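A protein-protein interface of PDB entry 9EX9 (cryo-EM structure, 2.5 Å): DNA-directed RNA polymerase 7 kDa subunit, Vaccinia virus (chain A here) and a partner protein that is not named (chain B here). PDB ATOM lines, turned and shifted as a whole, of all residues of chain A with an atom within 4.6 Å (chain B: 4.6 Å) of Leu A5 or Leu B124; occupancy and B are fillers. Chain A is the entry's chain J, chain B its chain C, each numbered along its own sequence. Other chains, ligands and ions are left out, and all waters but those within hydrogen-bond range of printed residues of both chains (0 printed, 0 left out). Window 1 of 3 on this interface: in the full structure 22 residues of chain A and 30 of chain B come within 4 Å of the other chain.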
ATOM      1  N   VAL A   2      24.469 -31.822  23.689  1.00  0.00           N
ATOM      2  CA  VAL A   2      25.480 -31.005  24.340  1.00  0.00           C
ATOM      3  C   VAL A   2      25.461 -29.595  23.764  1.00  0.00           C
ATOM      4  O   VAL A   2      26.337 -28.786  24.036  1.00  0.00           O
ATOM      5  CB  VAL A   2      26.859 -31.649  24.201  1.00  0.00           C
ATOM      6  CG1 VAL A   2      27.935 -30.779  24.822  1.00  0.00           C
ATOM      7  CG2 VAL A   2      26.846 -33.017  24.842  1.00  0.00           C
ATOM      8  N   PHE A   3      24.420 -29.297  22.993  1.00  0.00           N
ATOM      9  CA  PHE A   3      24.355 -28.097  22.175  1.00  0.00           C
ATOM     10  C   PHE A   3      23.315 -27.101  22.662  1.00  0.00           C
ATOM     11  O   PHE A   3      23.627 -25.922  22.840  1.00  0.00           O
ATOM     12  CB  PHE A   3      24.061 -28.506  20.727  1.00  0.00           C
ATOM     13  CG  PHE A   3      24.887 -27.788  19.707  1.00  0.00           C
ATOM     14  CD1 PHE A   3      26.166 -28.203  19.420  1.00  0.00           C
ATOM     15  CD2 PHE A   3      24.372 -26.708  19.014  1.00  0.00           C
ATOM     16  CE1 PHE A   3      26.918 -27.545  18.474  1.00  0.00           C
ATOM     17  CE2 PHE A   3      25.123 -26.052  18.071  1.00  0.00           C
ATOM     18  CZ  PHE A   3      26.393 -26.473  17.799  1.00  0.00           C
ATOM     19  N   GLN A   4      22.079 -27.541  22.885  1.00  0.00           N
ATOM     20  CA  GLN A   4      21.044 -26.642  23.378  1.00  0.00           C
ATOM     21  C   GLN A   4      21.413 -26.111  24.755  1.00  0.00           C
ATOM     22  O   GLN A   4      22.022 -26.805  25.571  1.00  0.00           O
ATOM     23  CB  GLN A   4      19.703 -27.363  23.446  1.00  0.00           C
ATOM     24  CG  GLN A   4      18.974 -27.454  22.136  1.00  0.00           C
ATOM     25  CD  GLN A   4      17.785 -28.377  22.210  1.00  0.00           C
ATOM     26  OE1 GLN A   4      17.785 -29.341  22.966  1.00  0.00           O
ATOM     27  NE2 GLN A   4      16.759 -28.084  21.433  1.00  0.00           N
ATOM     28  N   LEU A   5      21.034 -24.863  25.016  1.00  0.00           N
ATOM     29  CA  LEU A   5      21.368 -24.201  26.268  1.00  0.00           C
ATOM     30  C   LEU A   5      20.220 -24.183  27.267  1.00  0.00           C
ATOM     31  O   LEU A   5      20.428 -23.769  28.409  1.00  0.00           O
ATOM     32  CB  LEU A   5      21.823 -22.765  25.994  1.00  0.00           C
ATOM     33  CG  LEU A   5      23.102 -22.635  25.170  1.00  0.00           C
ATOM     34  CD1 LEU A   5      23.096 -21.351  24.395  1.00  0.00           C
ATOM     35  CD2 LEU A   5      24.312 -22.684  26.069  1.00  0.00           C
ATOM     36  N   VAL A   6      19.026 -24.626  26.876  1.00  0.00           N
ATOM     37  CA  VAL A   6      17.872 -24.670  27.761  1.00  0.00           C
ATOM     38  C   VAL A   6      17.200 -26.030  27.625  1.00  0.00           C
ATOM     39  O   VAL A   6      17.444 -26.779  26.679  1.00  0.00           O
ATOM     40  CB  VAL A   6      16.859 -23.543  27.460  1.00  0.00           C
ATOM     41  CG1 VAL A   6      17.492 -22.190  27.670  1.00  0.00           C
ATOM     42  CG2 VAL A   6      16.321 -23.666  26.051  1.00  0.00           C
ATOM     43  N   LYS A  12      14.240 -24.205  31.192  1.00  0.00           N
ATOM     44  CA  LYS A  12      15.224 -23.839  32.195  1.00  0.00           C
ATOM     45  C   LYS A  12      16.638 -23.889  31.624  1.00  0.00           C
ATOM     46  O   LYS A  12      16.898 -24.490  30.582  1.00  0.00           O
ATOM     47  CB  LYS A  12      15.128 -24.758  33.409  1.00  0.00           C
ATOM     48  CG  LYS A  12      14.156 -24.280  34.461  1.00  0.00           C
ATOM     49  CD  LYS A  12      14.311 -25.047  35.752  1.00  0.00           C
ATOM     50  CE  LYS A  12      13.600 -24.357  36.897  1.00  0.00           C
ATOM     51  NZ  LYS A  12      12.151 -24.181  36.644  1.00  0.00           N
ATOM     52  N   ASP A  13      17.557 -23.253  32.344  1.00  0.00           N
ATOM     53  CA  ASP A  13      18.944 -23.099  31.925  1.00  0.00           C
ATOM     54  C   ASP A  13      19.782 -24.259  32.453  1.00  0.00           C
ATOM     55  O   ASP A  13      19.824 -24.498  33.662  1.00  0.00           O
ATOM     56  CB  ASP A  13      19.476 -21.764  32.446  1.00  0.00           C
ATOM     57  CG  ASP A  13      20.928 -21.538  32.130  1.00  0.00           C
ATOM     58  OD1 ASP A  13      21.534 -22.369  31.431  1.00  0.00           O
ATOM     59  OD2 ASP A  13      21.471 -20.516  32.586  1.00  0.00           O
ATOM     60  N   ILE A  14      20.458 -24.969  31.547  1.00  0.00           N
ATOM     61  CA  ILE A  14      21.218 -26.159  31.918  1.00  0.00           C
ATOM     62  C   ILE A  14      22.646 -26.111  31.388  1.00  0.00           C
ATOM     63  O   ILE A  14      23.286 -27.154  31.232  1.00  0.00           O
ATOM     64  CB  ILE A  14      20.520 -27.433  31.412  1.00  0.00           C
ATOM     65  CG1 ILE A  14      20.394 -27.403  29.890  1.00  0.00           C
ATOM     66  CG2 ILE A  14      19.164 -27.592  32.068  1.00  0.00           C
ATOM     67  CD1 ILE A  14      19.753 -28.631  29.314  1.00  0.00           C
ATOM     68  N   SER A  15      23.162 -24.917  31.109  1.00  0.00           N
ATOM     69  CA  SER A  15      24.495 -24.826  30.520  1.00  0.00           C
ATOM     70  C   SER A  15      25.589 -25.053  31.558  1.00  0.00           C
ATOM     71  O   SER A  15      26.617 -25.671  31.257  1.00  0.00           O
ATOM     72  CB  SER A  15      24.667 -23.475  29.835  1.00  0.00           C
ATOM     73  OG  SER A  15      24.268 -22.425  30.687  1.00  0.00           O
ATOM     74  N   ARG A  18      25.867 -28.695  32.175  1.00  0.00           N
ATOM     75  CA  ARG A  18      26.444 -29.346  31.007  1.00  0.00           C
ATOM     76  C   ARG A  18      27.958 -29.186  30.972  1.00  0.00           C
ATOM     77  O   ARG A  18      28.680 -30.136  30.654  1.00  0.00           O
ATOM     78  CB  ARG A  18      25.822 -28.785  29.737  1.00  0.00           C
ATOM     79  CG  ARG A  18      26.036 -29.658  28.546  1.00  0.00           C
ATOM     80  CD  ARG A  18      25.425 -29.049  27.321  1.00  0.00           C
ATOM     81  NE  ARG A  18      23.968 -29.105  27.292  1.00  0.00           N
ATOM     82  CZ  ARG A  18      23.249 -30.214  27.188  1.00  0.00           C
ATOM     83  NH1 ARG A  18      23.808 -31.409  27.218  1.00  0.00           N
ATOM     84  NH2 ARG A  18      21.932 -30.122  27.054  1.00  0.00           N
ATOM     85  N   TYR A  19      28.463 -27.990  31.282  1.00  0.00           N
ATOM     86  CA  TYR A  19      29.910 -27.837  31.397  1.00  0.00           C
ATOM     87  C   TYR A  19      30.461 -28.711  32.511  1.00  0.00           C
ATOM     88  O   TYR A  19      31.480 -29.385  32.334  1.00  0.00           O
ATOM     89  CB  TYR A  19      30.278 -26.378  31.650  1.00  0.00           C
ATOM     90  CG  TYR A  19      31.748 -26.159  31.943  1.00  0.00           C
ATOM     91  CD1 TYR A  19      32.246 -26.281  33.229  1.00  0.00           C
ATOM     92  CD2 TYR A  19      32.633 -25.826  30.934  1.00  0.00           C
ATOM     93  CE1 TYR A  19      33.577 -26.082  33.498  1.00  0.00           C
ATOM     94  CE2 TYR A  19      33.968 -25.622  31.198  1.00  0.00           C
ATOM     95  CZ  TYR A  19      34.433 -25.752  32.480  1.00  0.00           C
ATOM     96  OH  TYR A  19      35.763 -25.551  32.745  1.00  0.00           O
ATOM     97  N   ILE A  22      30.463 -32.426  30.990  1.00  0.00           N
ATOM     98  CA  ILE A  22      31.208 -32.819  29.798  1.00  0.00           C
ATOM     99  C   ILE A  22      32.685 -32.466  29.920  1.00  0.00           C
ATOM    100  O   ILE A  22      33.549 -33.232  29.490  1.00  0.00           O
ATOM    101  CB  ILE A  22      30.587 -32.176  28.548  1.00  0.00           C
ATOM    102  CG1 ILE A  22      29.113 -32.552  28.410  1.00  0.00           C
ATOM    103  CG2 ILE A  22      31.346 -32.601  27.314  1.00  0.00           C
ATOM    104  CD1 ILE A  22      28.872 -33.999  28.086  1.00  0.00           C
ATOM    105  N   ILE A  23      33.006 -31.304  30.480  1.00  0.00           N
ATOM    106  CA  ILE A  23      34.387 -30.831  30.493  1.00  0.00           C
ATOM    107  C   ILE A  23      35.114 -31.271  31.755  1.00  0.00           C
ATOM    108  O   ILE A  23      36.226 -31.800  31.687  1.00  0.00           O
ATOM    109  CB  ILE A  23      34.422 -29.298  30.333  1.00  0.00           C
ATOM    110  CG1 ILE A  23      33.679 -28.872  29.067  1.00  0.00           C
ATOM    111  CG2 ILE A  23      35.851 -28.808  30.288  1.00  0.00           C
ATOM    112  CD1 ILE A  23      34.182 -29.512  27.804  1.00  0.00           C
ATOM    113  N   ALA B  55      20.456 -22.933  18.230  1.00  0.00           N
ATOM    114  CA  ALA B  55      21.045 -23.004  19.562  1.00  0.00           C
ATOM    115  C   ALA B  55      21.255 -21.616  20.149  1.00  0.00           C
ATOM    116  O   ALA B  55      21.012 -21.398  21.341  1.00  0.00           O
ATOM    117  CB  ALA B  55      22.363 -23.769  19.508  1.00  0.00           C
ATOM    118  N   HIS B  58      18.199 -19.144  21.749  1.00  0.00           N
ATOM    119  CA  HIS B  58      17.667 -19.316  23.094  1.00  0.00           C
ATOM    120  C   HIS B  58      18.764 -19.217  24.142  1.00  0.00           C
ATOM    121  O   HIS B  58      18.777 -19.956  25.123  1.00  0.00           O
ATOM    122  CB  HIS B  58      16.926 -20.644  23.214  1.00  0.00           C
ATOM    123  CG  HIS B  58      15.713 -20.729  22.344  1.00  0.00           C
ATOM    124  ND1 HIS B  58      14.482 -20.257  22.736  1.00  0.00           N
ATOM    125  CD2 HIS B  58      15.547 -21.218  21.094  1.00  0.00           C
ATOM    126  CE1 HIS B  58      13.608 -20.453  21.767  1.00  0.00           C
ATOM    127  NE2 HIS B  58      14.229 -21.035  20.758  1.00  0.00           N
ATOM    128  N   ILE B  59      19.694 -18.294  23.954  1.00  0.00           N
ATOM    129  CA  ILE B  59      20.677 -18.015  25.005  1.00  0.00           C
ATOM    130  C   ILE B  59      19.977 -17.304  26.158  1.00  0.00           C
ATOM    131  O   ILE B  59      19.258 -16.320  25.923  1.00  0.00           O
ATOM    132  CB  ILE B  59      21.818 -17.163  24.456  1.00  0.00           C
ATOM    133  CG1 ILE B  59      22.643 -17.965  23.453  1.00  0.00           C
ATOM    134  CG2 ILE B  59      22.688 -16.652  25.595  1.00  0.00           C
ATOM    135  CD1 ILE B  59      23.743 -17.179  22.806  1.00  0.00           C
ATOM    136  N   PRO B  60      20.157 -17.736  27.405  1.00  0.00           N
ATOM    137  CA  PRO B  60      19.517 -17.028  28.521  1.00  0.00           C
ATOM    138  C   PRO B  60      20.189 -15.700  28.826  1.00  0.00           C
ATOM    139  O   PRO B  60      21.078 -15.625  29.678  1.00  0.00           O
ATOM    140  CB  PRO B  60      19.654 -18.015  29.685  1.00  0.00           C
ATOM    141  CG  PRO B  60      20.815 -18.841  29.339  1.00  0.00           C
ATOM    142  CD  PRO B  60      20.823 -18.968  27.854  1.00  0.00           C
ATOM    143  N   TYR B  93      36.946 -25.763  22.844  1.00  0.00           N
ATOM    144  CA  TYR B  93      35.495 -25.706  22.957  1.00  0.00           C
ATOM    145  C   TYR B  93      35.068 -24.253  23.097  1.00  0.00           C
ATOM    146  O   TYR B  93      35.894 -23.355  23.273  1.00  0.00           O
ATOM    147  CB  TYR B  93      34.993 -26.542  24.137  1.00  0.00           C
ATOM    148  CG  TYR B  93      35.686 -26.235  25.440  1.00  0.00           C
ATOM    149  CD1 TYR B  93      35.313 -25.146  26.203  1.00  0.00           C
ATOM    150  CD2 TYR B  93      36.709 -27.040  25.908  1.00  0.00           C
ATOM    151  CE1 TYR B  93      35.943 -24.863  27.388  1.00  0.00           C
ATOM    152  CE2 TYR B  93      37.342 -26.763  27.093  1.00  0.00           C
ATOM    153  CZ  TYR B  93      36.955 -25.674  27.829  1.00  0.00           C
ATOM    154  OH  TYR B  93      37.584 -25.392  29.014  1.00  0.00           O
ATOM    155  N   ILE B  94      33.759 -24.035  23.017  1.00  0.00           N
ATOM    156  CA  ILE B  94      33.161 -22.707  23.068  1.00  0.00           C
ATOM    157  C   ILE B  94      32.266 -22.621  24.297  1.00  0.00           C
ATOM    158  O   ILE B  94      31.402 -23.479  24.502  1.00  0.00           O
ATOM    159  CB  ILE B  94      32.357 -22.405  21.793  1.00  0.00           C
ATOM    160  CG1 ILE B  94      33.228 -22.616  20.560  1.00  0.00           C
ATOM    161  CG2 ILE B  94      31.834 -20.985  21.824  1.00  0.00           C
ATOM    162  CD1 ILE B  94      32.499 -22.442  19.269  1.00  0.00           C
ATOM    163  N   LEU B  96      30.046 -19.597  26.972  1.00  0.00           N
ATOM    164  CA  LEU B  96      29.302 -18.350  26.837  1.00  0.00           C
ATOM    165  C   LEU B  96      30.153 -17.125  27.126  1.00  0.00           C
ATOM    166  O   LEU B  96      29.674 -16.002  26.946  1.00  0.00           O
ATOM    167  CB  LEU B  96      28.085 -18.340  27.765  1.00  0.00           C
ATOM    168  CG  LEU B  96      26.912 -19.250  27.402  1.00  0.00           C
ATOM    169  CD1 LEU B  96      25.782 -19.041  28.385  1.00  0.00           C
ATOM    170  CD2 LEU B  96      26.431 -19.001  25.990  1.00  0.00           C
ATOM    171  N   GLU B 122      32.481 -21.140  32.709  1.00  0.00           N
ATOM    172  CA  GLU B 122      32.157 -22.529  33.007  1.00  0.00           C
ATOM    173  C   GLU B 122      30.777 -22.904  32.482  1.00  0.00           C
ATOM    174  O   GLU B 122      29.967 -23.506  33.184  1.00  0.00           O
ATOM    175  CB  GLU B 122      32.257 -22.800  34.501  1.00  0.00           C
ATOM    176  CG  GLU B 122      33.662 -22.649  35.035  1.00  0.00           C
ATOM    177  CD  GLU B 122      33.893 -23.439  36.304  1.00  0.00           C
ATOM    178  OE1 GLU B 122      32.950 -24.105  36.776  1.00  0.00           O
ATOM    179  OE2 GLU B 122      35.024 -23.400  36.829  1.00  0.00           O
ATOM    180  N   THR B 123      30.500 -22.529  31.242  1.00  0.00           N
ATOM    181  CA  THR B 123      29.332 -22.979  30.507  1.00  0.00           C
ATOM    182  C   THR B 123      29.803 -23.606  29.203  1.00  0.00           C
ATOM    183  O   THR B 123      30.911 -23.340  28.738  1.00  0.00           O
ATOM    184  CB  THR B 123      28.375 -21.818  30.236  1.00  0.00           C
ATOM    185  OG1 THR B 123      29.056 -20.800  29.501  1.00  0.00           O
ATOM    186  CG2 THR B 123      27.888 -21.231  31.536  1.00  0.00           C
ATOM    187  N   LEU B 124      28.971 -24.461  28.616  1.00  0.00           N
ATOM    188  CA  LEU B 124      29.363 -25.194  27.423  1.00  0.00           C
ATOM    189  C   LEU B 124      28.322 -25.045  26.329  1.00  0.00           C
ATOM    190  O   LEU B 124      27.121 -25.154  26.583  1.00  0.00           O
ATOM    191  CB  LEU B 124      29.567 -26.674  27.723  1.00  0.00           C
ATOM    192  CG  LEU B 124      30.015 -27.516  26.528  1.00  0.00           C
ATOM    193  CD1 LEU B 124      31.334 -27.015  25.996  1.00  0.00           C
ATOM    194  CD2 LEU B 124      30.120 -28.967  26.914  1.00  0.00           C
ATOM    195  N   LEU B 125      28.798 -24.811  25.108  1.00  0.00           N
ATOM    196  CA  LEU B 125      27.963 -24.737  23.916  1.00  0.00           C
ATOM    197  C   LEU B 125      28.386 -25.704  22.824  1.00  0.00           C
ATOM    198  O   LEU B 125      27.527 -26.312  22.188  1.00  0.00           O
ATOM    199  CB  LEU B 125      27.979 -23.308  23.354  1.00  0.00           C
ATOM    200  CG  LEU B 125      27.293 -23.093  22.000  1.00  0.00           C
ATOM    201  CD1 LEU B 125      25.813 -23.388  22.084  1.00  0.00           C
ATOM    202  CD2 LEU B 125      27.518 -21.685  21.503  1.00  0.00           C
ATOM    203  N   HIS B 126      29.686 -25.866  22.583  1.00  0.00           N
ATOM    204  CA  HIS B 126      30.161 -26.648  21.449  1.00  0.00           C
ATOM    205  C   HIS B 126      31.560 -27.158  21.745  1.00  0.00           C
ATOM    206  O   HIS B 126      32.374 -26.440  22.326  1.00  0.00           O
ATOM    207  CB  HIS B 126      30.165 -25.807  20.169  1.00  0.00           C
ATOM    208  CG  HIS B 126      30.724 -26.513  18.973  1.00  0.00           C
ATOM    209  ND1 HIS B 126      30.074 -27.556  18.351  1.00  0.00           N
ATOM    210  CD2 HIS B 126      31.865 -26.313  18.274  1.00  0.00           C
ATOM    211  CE1 HIS B 126      30.793 -27.972  17.325  1.00  0.00           C
ATOM    212  NE2 HIS B 126      31.886 -27.235  17.257  1.00  0.00           N
ATOM    213  N   VAL B 127      31.831 -28.393  21.334  1.00  0.00           N
ATOM    214  CA  VAL B 127      33.140 -29.015  21.495  1.00  0.00           C
ATOM    215  C   VAL B 127      33.698 -29.294  20.108  1.00  0.00           C
ATOM    216  O   VAL B 127      33.076 -30.013  19.318  1.00  0.00           O
ATOM    217  CB  VAL B 127      33.065 -30.308  22.321  1.00  0.00           C
ATOM    218  CG1 VAL B 127      34.438 -30.915  22.471  1.00  0.00           C
ATOM    219  CG2 VAL B 127      32.470 -30.031  23.683  1.00  0.00           C
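Of the 13 printed residues of chain B, 9 touch a printed residue of chain A. Of the 13 printed residues of chain A, 8 touch a printed residue of chain B.
Among the printed residues, merely in contact across the chains: Val A2 with Leu B124 (3.5 Å), Phe A3 with Ala B55 (3.6 Å), Phe A3 with Leu B125 (3.4 Å), Phe A3 with His B126 (3.2 Å), Leu A5 with Ala B55 (3.7 Å), Leu A5 with Ile B59 (3.5 Å), Leu A5 with Leu B124 (3.8 Å), Val A6 with His B58 (3.6 Å), Asp A13 with Pro B60 (3.7 Å), Ser A15 with Thr B123 (3.9 Å), Ser A15 with Leu B124 (3.7 Å), Tyr A19 with Glu B122 (3.3 Å), Tyr A19 with Thr B123 (3.7 Å), Tyr A19 with Leu B124 (3.8 Å) and Ile A22 with Leu B124 (3.6 Å).
The backbone NH of Leu B125 is in hydrogen-bond range of the backbone carbonyl oxygen of Ile B94 (3.0 Å). The backbone NH of Ile B94 sits at hydrogen-bond distance from the backbone carbonyl oxygen of His B126, at 2.9 Å. N of Leu B96 is in hydrogen-bond range of OG1 of Thr B123. O of Leu A5 is in hydrogen-bond range of N of Ile A14. The side-chain carboxylate (OD1) of Asp A13 sits at hydrogen-bond distance from the side-chain hydroxyl (OG) of Ser A15 (2.8 Å).
O of Val A2 sits close to O of Leu B125, 3.3 Å away.
Printed residues of chain B within 4 Å of Leu A5: Ala B55, Ile B59 and Leu B124. Lys A12 touches none of the printed residues of chain B. Arg A18 touches none of the printed residues of chain B. Of the printed residues of chain A, Ala B55 touches Phe A3 and Leu A5. Printed residues of chain A within 4 Å of His B58: Val A6 (3.6 Å). Printed residues of chain A within 4 Å of Glu B122: Tyr A19 (3.3 Å). The nearest residue of chain B that does not touch Leu A5 is Leu B125 (4.1 Å).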
